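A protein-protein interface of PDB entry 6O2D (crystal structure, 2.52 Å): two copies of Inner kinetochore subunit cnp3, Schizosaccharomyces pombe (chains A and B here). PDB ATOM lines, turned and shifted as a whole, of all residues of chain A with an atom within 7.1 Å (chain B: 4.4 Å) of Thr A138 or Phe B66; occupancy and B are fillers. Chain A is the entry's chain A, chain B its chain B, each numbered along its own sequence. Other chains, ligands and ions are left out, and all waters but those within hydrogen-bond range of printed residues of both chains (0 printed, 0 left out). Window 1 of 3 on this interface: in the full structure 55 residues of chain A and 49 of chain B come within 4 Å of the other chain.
O of Ser A65 sits at hydrogen-bond distance from N of Thr A141 (3.2 Å).
The backbone NH (N) of Ile A88 lies within hydrogen-bond range of the backbone carbonyl oxygen (O) of Ala A140 (2.7 Å).
The side-chain hydroxyl of Thr A138 lies within hydrogen-bond range of the side-chain hydroxyl of Ser A90 (2.9 Å).
CE1 of Phe A66 touches OG1 of Thr B138, at 3.8 Å.
Ile A88 touches Glu B62.
Ile A88 touches Ser B65.
Ile A88 touches Phe B66.
CB of Ser A90 touches CZ of Phe B66, at 3.98 Å.
Thr A138 touches Phe B66 (OG1 to CE1, 3.7 Å).
CB of Ala A140 touches CD1 of Phe B66 (3.5 Å).
Thr A141 touches Ser B65.
Asp A142 touches Pro B64 (OD2 to CD, 3.6 Å).
Ser B65 touches Asp A142 (CB to OD2, 3.7 Å).
Ser A65 touches none of the printed residues of chain B.
Printed residues of chain B within 4 Å of Ile A88: Glu B62, Ser B65 and Phe B66.
Printed residues of chain B within 4 Å of Thr A138: Phe B66 (3.7 Å).
Printed residues of chain A within 4 Å of Pro B64: Asp A142 (3.6 Å).
Of the printed residues of chain A, Phe B66 touches Ile A88, Ser A90, Ile A116, Thr A138 and Ala A140.
Of the printed residues of chain A, Thr B138 touches Phe A66.
The nearest printed residue of chain B that does not touch Thr A138 is Thr B138 (4.02 Å).
The nearest printed residue of chain A that does not touch Phe B66 is Phe A66 (4.9 Å).
The nearest printed residue of chain B that does not touch Phe A66 is Phe B66 (4.9 Å).
Of the 18 printed residues of chain A, 8 touch a printed residue of chain B.
Printed residues of chain A that touch a printed residue of chain B: Phe A66, Ile A88, Ser A90, Ile A116, Thr A138, Ala A140, Thr A141 and Asp A142.
Hydrophobic or aromatic side chains of chain A within 4 Å of the printed part of chain B: Phe A66, Ile A88, Ile A116 and Ala A140.
Hydrophobic or aromatic side chains of chain B that line the printed part of chain A: Pro B64 and Phe B66.
Among the printed residues, no Asp or Glu carboxylate lies within 4 Å of a Lys or Arg side-chain nitrogen of the other chain.
Phe A66 touches Thr B138, and with the chains exchanged Thr A138 touches Phe B66.
Positions printed for both chains: 65, 66, 67, 68, 138 and 139.
Of the 11 pairs that touch across the chains among the printed residues, 2 have their exchanged pair printed and touching as well.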
ATOM      1  N   SER A  65      -9.210   5.117   6.536  1.00  0.00           N
ATOM      2  CA  SER A  65     -10.190   5.496   5.522  1.00  0.00           C
ATOM      3  C   SER A  65     -10.397   7.000   5.370  1.00  0.00           C
ATOM      4  O   SER A  65     -10.800   7.438   4.290  1.00  0.00           O
ATOM      5  CB  SER A  65     -11.531   4.814   5.814  1.00  0.00           C
ATOM      6  OG  SER A  65     -12.271   5.551   6.774  1.00  0.00           O
ATOM      7  N   PHE A  66     -10.174   7.803   6.408  1.00  0.00           N
ATOM      8  CA  PHE A  66     -10.562   9.206   6.333  1.00  0.00           C
ATOM      9  C   PHE A  66      -9.589  10.095   7.099  1.00  0.00           C
ATOM     10  O   PHE A  66      -9.064   9.704   8.145  1.00  0.00           O
ATOM     11  CB  PHE A  66     -11.983   9.415   6.877  1.00  0.00           C
ATOM     12  CG  PHE A  66     -12.417  10.861   6.926  1.00  0.00           C
ATOM     13  CD1 PHE A  66     -12.871  11.501   5.780  1.00  0.00           C
ATOM     14  CD2 PHE A  66     -12.385  11.572   8.116  1.00  0.00           C
ATOM     15  CE1 PHE A  66     -13.276  12.816   5.821  1.00  0.00           C
ATOM     16  CE2 PHE A  66     -12.792  12.896   8.159  1.00  0.00           C
ATOM     17  CZ  PHE A  66     -13.238  13.514   7.014  1.00  0.00           C
ATOM     18  N   ALA A  67      -9.360  11.292   6.559  1.00  0.00           N
ATOM     19  CA  ALA A  67      -8.592  12.328   7.234  1.00  0.00           C
ATOM     20  C   ALA A  67      -9.168  13.684   6.851  1.00  0.00           C
ATOM     21  O   ALA A  67      -9.784  13.829   5.792  1.00  0.00           O
ATOM     22  CB  ALA A  67      -7.107  12.258   6.871  1.00  0.00           C
ATOM     23  N   ALA A  68      -8.998  14.667   7.737  1.00  0.00           N
ATOM     24  CA  ALA A  68      -9.438  16.027   7.445  1.00  0.00           C
ATOM     25  C   ALA A  68      -8.512  17.017   8.130  1.00  0.00           C
ATOM     26  O   ALA A  68      -7.913  16.714   9.166  1.00  0.00           O
ATOM     27  CB  ALA A  68     -10.880  16.290   7.887  1.00  0.00           C
ATOM     28  N   GLY A  69      -8.415  18.207   7.553  1.00  0.00           N
ATOM     29  CA  GLY A  69      -7.544  19.208   8.132  1.00  0.00           C
ATOM     30  C   GLY A  69      -7.802  20.578   7.555  1.00  0.00           C
ATOM     31  O   GLY A  69      -8.816  20.820   6.894  1.00  0.00           O
ATOM     32  N   ILE A  88      -9.258  10.087  -2.606  1.00  0.00           N
ATOM     33  CA  ILE A  88     -10.182  11.130  -3.032  1.00  0.00           C
ATOM     34  C   ILE A  88      -9.960  12.327  -2.129  1.00  0.00           C
ATOM     35  O   ILE A  88     -10.042  12.207  -0.903  1.00  0.00           O
ATOM     36  CB  ILE A  88     -11.640  10.655  -2.931  1.00  0.00           C
ATOM     37  CG1 ILE A  88     -11.784   9.236  -3.481  1.00  0.00           C
ATOM     38  CG2 ILE A  88     -12.566  11.639  -3.648  1.00  0.00           C
ATOM     39  CD1 ILE A  88     -12.744   8.375  -2.688  1.00  0.00           C
ATOM     40  N   MET A  89      -9.677  13.481  -2.717  1.00  0.00           N
ATOM     41  CA  MET A  89      -9.578  14.681  -1.907  1.00  0.00           C
ATOM     42  C   MET A  89     -10.687  15.649  -2.252  1.00  0.00           C
ATOM     43  O   MET A  89     -11.096  15.746  -3.402  1.00  0.00           O
ATOM     44  CB  MET A  89      -8.217  15.343  -2.075  1.00  0.00           C
ATOM     45  CG  MET A  89      -7.075  14.514  -1.516  1.00  0.00           C
ATOM     46  SD  MET A  89      -5.512  14.698  -2.620  1.00  0.00           S
ATOM     47  CE  MET A  89      -4.568  16.094  -1.738  1.00  0.00           C
ATOM     48  N   SER A  90     -11.187  16.336  -1.231  1.00  0.00           N
ATOM     49  CA  SER A  90     -12.197  17.369  -1.375  1.00  0.00           C
ATOM     50  C   SER A  90     -11.708  18.590  -0.622  1.00  0.00           C
ATOM     51  O   SER A  90     -11.007  18.463   0.387  1.00  0.00           O
ATOM     52  CB  SER A  90     -13.563  16.908  -0.858  1.00  0.00           C
ATOM     53  OG  SER A  90     -13.766  17.287   0.494  1.00  0.00           O
ATOM     54  N   PHE A  91     -12.035  19.768  -1.144  1.00  0.00           N
ATOM     55  CA  PHE A  91     -11.604  21.035  -0.571  1.00  0.00           C
ATOM     56  C   PHE A  91     -12.800  21.965  -0.503  1.00  0.00           C
ATOM     57  O   PHE A  91     -13.568  22.078  -1.465  1.00  0.00           O
ATOM     58  CB  PHE A  91     -10.494  21.687  -1.391  1.00  0.00           C
ATOM     59  CG  PHE A  91      -9.251  20.843  -1.531  1.00  0.00           C
ATOM     60  CD1 PHE A  91      -8.151  21.044  -0.704  1.00  0.00           C
ATOM     61  CD2 PHE A  91      -9.176  19.857  -2.504  1.00  0.00           C
ATOM     62  CE1 PHE A  91      -6.999  20.265  -0.843  1.00  0.00           C
ATOM     63  CE2 PHE A  91      -8.030  19.080  -2.656  1.00  0.00           C
ATOM     64  CZ  PHE A  91      -6.939  19.283  -1.822  1.00  0.00           C
ATOM     65  N   CYS A  92     -12.937  22.636   0.633  1.00  0.00           N
ATOM     66  CA  CYS A  92     -13.942  23.664   0.844  1.00  0.00           C
ATOM     67  C   CYS A  92     -13.217  24.979   1.116  1.00  0.00           C
ATOM     68  O   CYS A  92     -12.337  25.019   1.981  1.00  0.00           O
ATOM     69  CB  CYS A  92     -14.823  23.253   2.035  1.00  0.00           C
ATOM     70  SG  CYS A  92     -16.162  24.354   2.385  1.00  0.00           S
ATOM     71  N   ILE A 116     -13.298  18.689  -5.803  1.00  0.00           N
ATOM     72  CA  ILE A 116     -12.763  17.371  -5.505  1.00  0.00           C
ATOM     73  C   ILE A 116     -11.601  17.091  -6.452  1.00  0.00           C
ATOM     74  O   ILE A 116     -11.583  17.557  -7.595  1.00  0.00           O
ATOM     75  CB  ILE A 116     -13.882  16.303  -5.629  1.00  0.00           C
ATOM     76  CG1 ILE A 116     -13.528  15.021  -4.887  1.00  0.00           C
ATOM     77  CG2 ILE A 116     -14.217  15.981  -7.096  1.00  0.00           C
ATOM     78  CD1 ILE A 116     -14.707  14.395  -4.187  1.00  0.00           C
ATOM     79  N   TYR A 136     -10.579  23.942   4.105  1.00  0.00           N
ATOM     80  CA  TYR A 136     -10.866  22.738   4.856  1.00  0.00           C
ATOM     81  C   TYR A 136     -10.775  21.600   3.857  1.00  0.00           C
ATOM     82  O   TYR A 136     -11.458  21.627   2.827  1.00  0.00           O
ATOM     83  CB  TYR A 136     -12.251  22.785   5.500  1.00  0.00           C
ATOM     84  CG  TYR A 136     -12.663  21.461   6.086  1.00  0.00           C
ATOM     85  CD1 TYR A 136     -12.024  20.951   7.208  1.00  0.00           C
ATOM     86  CD2 TYR A 136     -13.677  20.710   5.510  1.00  0.00           C
ATOM     87  CE1 TYR A 136     -12.394  19.730   7.747  1.00  0.00           C
ATOM     88  CE2 TYR A 136     -14.057  19.487   6.041  1.00  0.00           C
ATOM     89  CZ  TYR A 136     -13.409  19.005   7.157  1.00  0.00           C
ATOM     90  OH  TYR A 136     -13.773  17.788   7.683  1.00  0.00           O
ATOM     91  N   TYR A 137      -9.898  20.641   4.120  1.00  0.00           N
ATOM     92  CA  TYR A 137      -9.716  19.514   3.221  1.00  0.00           C
ATOM     93  C   TYR A 137     -10.125  18.222   3.914  1.00  0.00           C
ATOM     94  O   TYR A 137     -10.121  18.123   5.144  1.00  0.00           O
ATOM     95  CB  TYR A 137      -8.266  19.415   2.712  1.00  0.00           C
ATOM     96  CG  TYR A 137      -7.250  18.922   3.721  1.00  0.00           C
ATOM     97  CD1 TYR A 137      -6.991  17.562   3.876  1.00  0.00           C
ATOM     98  CD2 TYR A 137      -6.529  19.819   4.502  1.00  0.00           C
ATOM     99  CE1 TYR A 137      -6.057  17.111   4.792  1.00  0.00           C
ATOM    100  CE2 TYR A 137      -5.586  19.377   5.412  1.00  0.00           C
ATOM    101  CZ  TYR A 137      -5.360  18.023   5.560  1.00  0.00           C
ATOM    102  OH  TYR A 137      -4.428  17.578   6.473  1.00  0.00           O
ATOM    103  N   THR A 138     -10.527  17.254   3.104  1.00  0.00           N
ATOM    104  CA  THR A 138     -10.720  15.879   3.526  1.00  0.00           C
ATOM    105  C   THR A 138     -10.071  14.995   2.482  1.00  0.00           C
ATOM    106  O   THR A 138     -10.083  15.331   1.295  1.00  0.00           O
ATOM    107  CB  THR A 138     -12.200  15.492   3.638  1.00  0.00           C
ATOM    108  OG1 THR A 138     -12.736  15.299   2.323  1.00  0.00           O
ATOM    109  CG2 THR A 138     -13.004  16.562   4.370  1.00  0.00           C
ATOM    110  N   HIS A 139      -9.482  13.885   2.903  1.00  0.00           N
ATOM    111  CA  HIS A 139      -9.160  12.868   1.918  1.00  0.00           C
ATOM    112  C   HIS A 139      -9.625  11.509   2.406  1.00  0.00           C
ATOM    113  O   HIS A 139      -9.579  11.200   3.597  1.00  0.00           O
ATOM    114  CB  HIS A 139      -7.670  12.859   1.517  1.00  0.00           C
ATOM    115  CG  HIS A 139      -6.716  12.534   2.619  1.00  0.00           C
ATOM    116  ND1 HIS A 139      -6.436  11.242   3.003  1.00  0.00           N
ATOM    117  CD2 HIS A 139      -5.923  13.332   3.371  1.00  0.00           C
ATOM    118  CE1 HIS A 139      -5.539  11.259   3.972  1.00  0.00           C
ATOM    119  NE2 HIS A 139      -5.210  12.515   4.214  1.00  0.00           N
ATOM    120  N   ALA A 140     -10.067  10.700   1.461  1.00  0.00           N
ATOM    121  CA  ALA A 140     -10.734   9.453   1.752  1.00  0.00           C
ATOM    122  C   ALA A 140     -10.212   8.419   0.771  1.00  0.00           C
ATOM    123  O   ALA A 140      -9.702   8.758  -0.297  1.00  0.00           O
ATOM    124  CB  ALA A 140     -12.256   9.617   1.649  1.00  0.00           C
ATOM    125  N   THR A 141     -10.311   7.151   1.153  1.00  0.00           N
ATOM    126  CA  THR A 141      -9.815   6.087   0.295  1.00  0.00           C
ATOM    127  C   THR A 141     -10.711   4.867   0.459  1.00  0.00           C
ATOM    128  O   THR A 141     -11.369   4.697   1.489  1.00  0.00           O
ATOM    129  CB  THR A 141      -8.349   5.759   0.631  1.00  0.00           C
ATOM    130  OG1 THR A 141      -7.791   4.898  -0.370  1.00  0.00           O
ATOM    131  CG2 THR A 141      -8.248   5.079   1.996  1.00  0.00           C
ATOM    132  N   ASP A 142     -10.744   4.027  -0.573  1.00  0.00           N
ATOM    133  CA  ASP A 142     -11.562   2.817  -0.582  1.00  0.00           C
ATOM    134  C   ASP A 142     -10.671   1.655  -0.143  1.00  0.00           C
ATOM    135  O   ASP A 142      -9.934   1.083  -0.951  1.00  0.00           O
ATOM    136  CB  ASP A 142     -12.169   2.595  -1.962  1.00  0.00           C
ATOM    137  CG  ASP A 142     -13.165   1.463  -1.982  1.00  0.00           C
ATOM    138  OD1 ASP A 142     -12.775   0.338  -1.614  1.00  0.00           O
ATOM    139  OD2 ASP A 142     -14.333   1.693  -2.368  1.00  0.00           O
ATOM    140  N   LYS B  61     -19.936  12.225  -5.403  1.00  0.00           N
ATOM    141  CA  LYS B  61     -20.222  10.856  -4.998  1.00  0.00           C
ATOM    142  C   LYS B  61     -19.073   9.958  -5.418  1.00  0.00           C
ATOM    143  O   LYS B  61     -18.766   9.852  -6.611  1.00  0.00           O
ATOM    144  CB  LYS B  61     -21.525  10.368  -5.627  1.00  0.00           C
ATOM    145  CG  LYS B  61     -22.760  11.108  -5.155  1.00  0.00           C
ATOM    146  CD  LYS B  61     -24.025  10.480  -5.720  1.00  0.00           C
ATOM    147  CE  LYS B  61     -24.355  11.017  -7.104  1.00  0.00           C
ATOM    148  NZ  LYS B  61     -25.609  10.406  -7.630  1.00  0.00           N
ATOM    149  N   GLU B  62     -18.471   9.274  -4.447  1.00  0.00           N
ATOM    150  CA  GLU B  62     -17.531   8.201  -4.735  1.00  0.00           C
ATOM    151  C   GLU B  62     -18.024   6.939  -4.027  1.00  0.00           C
ATOM    152  O   GLU B  62     -17.461   6.510  -3.018  1.00  0.00           O
ATOM    153  CB  GLU B  62     -16.115   8.566  -4.300  1.00  0.00           C
ATOM    154  CG  GLU B  62     -15.055   7.684  -4.934  1.00  0.00           C
ATOM    155  CD  GLU B  62     -14.935   7.905  -6.424  1.00  0.00           C
ATOM    156  OE1 GLU B  62     -14.544   9.020  -6.826  1.00  0.00           O
ATOM    157  OE2 GLU B  62     -15.242   6.968  -7.190  1.00  0.00           O
ATOM    158  N   GLU B  63     -19.101   6.365  -4.559  1.00  0.00           N
ATOM    159  CA  GLU B  63     -19.674   5.165  -3.970  1.00  0.00           C
ATOM    160  C   GLU B  63     -18.669   4.019  -4.062  1.00  0.00           C
ATOM    161  O   GLU B  63     -17.987   3.867  -5.080  1.00  0.00           O
ATOM    162  CB  GLU B  63     -20.980   4.784  -4.665  1.00  0.00           C
ATOM    163  CG  GLU B  63     -22.223   5.275  -3.936  1.00  0.00           C
ATOM    164  CD  GLU B  63     -22.688   4.323  -2.844  1.00  0.00           C
ATOM    165  OE1 GLU B  63     -22.900   4.780  -1.702  1.00  0.00           O
ATOM    166  OE2 GLU B  63     -22.843   3.114  -3.126  1.00  0.00           O
ATOM    167  N   PRO B  64     -18.561   3.184  -3.025  1.00  0.00           N
ATOM    168  CA  PRO B  64     -19.298   3.300  -1.762  1.00  0.00           C
ATOM    169  C   PRO B  64     -18.523   3.968  -0.623  1.00  0.00           C
ATOM    170  O   PRO B  64     -19.032   4.020   0.493  1.00  0.00           O
ATOM    171  CB  PRO B  64     -19.600   1.843  -1.412  1.00  0.00           C
ATOM    172  CG  PRO B  64     -18.460   1.065  -2.018  1.00  0.00           C
ATOM    173  CD  PRO B  64     -17.871   1.885  -3.146  1.00  0.00           C
ATOM    174  N   SER B  65     -17.322   4.478  -0.886  1.00  0.00           N
ATOM    175  CA  SER B  65     -16.439   4.892   0.201  1.00  0.00           C
ATOM    176  C   SER B  65     -16.627   6.343   0.654  1.00  0.00           C
ATOM    177  O   SER B  65     -16.384   6.640   1.831  1.00  0.00           O
ATOM    178  CB  SER B  65     -14.977   4.638  -0.203  1.00  0.00           C
ATOM    179  OG  SER B  65     -14.364   5.787  -0.760  1.00  0.00           O
ATOM    180  N   PHE B  66     -17.039   7.260  -0.224  1.00  0.00           N
ATOM    181  CA  PHE B  66     -17.048   8.677   0.134  1.00  0.00           C
ATOM    182  C   PHE B  66     -18.175   9.403  -0.587  1.00  0.00           C
ATOM    183  O   PHE B  66     -18.471   9.105  -1.745  1.00  0.00           O
ATOM    184  CB  PHE B  66     -15.691   9.308  -0.202  1.00  0.00           C
ATOM    185  CG  PHE B  66     -15.645  10.810  -0.067  1.00  0.00           C
ATOM    186  CD1 PHE B  66     -15.280  11.397   1.137  1.00  0.00           C
ATOM    187  CD2 PHE B  66     -15.916  11.634  -1.161  1.00  0.00           C
ATOM    188  CE1 PHE B  66     -15.213  12.780   1.266  1.00  0.00           C
ATOM    189  CE2 PHE B  66     -15.858  13.015  -1.041  1.00  0.00           C
ATOM    190  CZ  PHE B  66     -15.506  13.589   0.179  1.00  0.00           C
ATOM    191  N   ALA B  67     -18.798  10.358   0.105  1.00  0.00           N
ATOM    192  CA  ALA B  67     -19.785  11.252  -0.493  1.00  0.00           C
ATOM    193  C   ALA B  67     -19.694  12.606   0.200  1.00  0.00           C
ATOM    194  O   ALA B  67     -19.283  12.690   1.360  1.00  0.00           O
ATOM    195  CB  ALA B  67     -21.208  10.690  -0.392  1.00  0.00           C
ATOM    196  N   ALA B  68     -20.061  13.669  -0.520  1.00  0.00           N
ATOM    197  CA  ALA B  68     -20.030  15.012   0.052  1.00  0.00           C
ATOM    198  C   ALA B  68     -21.118  15.889  -0.559  1.00  0.00           C
ATOM    199  O   ALA B  68     -21.528  15.695  -1.710  1.00  0.00           O
ATOM    200  CB  ALA B  68     -18.656  15.665  -0.132  1.00  0.00           C
ATOM    201  N   THR B 138     -19.261  15.872   4.591  1.00  0.00           N
ATOM    202  CA  THR B 138     -18.693  14.680   3.983  1.00  0.00           C
ATOM    203  C   THR B 138     -19.013  13.513   4.900  1.00  0.00           C
ATOM    204  O   THR B 138     -18.994  13.662   6.125  1.00  0.00           O
ATOM    205  CB  THR B 138     -17.170  14.800   3.771  1.00  0.00           C
ATOM    206  OG1 THR B 138     -16.498  14.693   5.027  1.00  0.00           O
ATOM    207  CG2 THR B 138     -16.804  16.150   3.140  1.00  0.00           C
ATOM    208  N   HIS B 139     -19.309  12.357   4.316  1.00  0.00           N
ATOM    209  CA  HIS B 139     -19.331  11.121   5.080  1.00  0.00           C
ATOM    210  C   HIS B 139     -18.519  10.065   4.349  1.00  0.00           C
ATOM    211  O   HIS B 139     -18.382  10.097   3.123  1.00  0.00           O
ATOM    212  CB  HIS B 139     -20.760  10.614   5.375  1.00  0.00           C
ATOM    213  CG  HIS B 139     -21.579  10.314   4.164  1.00  0.00           C
ATOM    214  ND1 HIS B 139     -22.544  11.177   3.690  1.00  0.00           N
ATOM    215  CD2 HIS B 139     -21.613   9.230   3.354  1.00  0.00           C
ATOM    216  CE1 HIS B 139     -23.118  10.650   2.624  1.00  0.00           C
ATOM    217  NE2 HIS B 139     -22.571   9.469   2.398  1.00  0.00           N
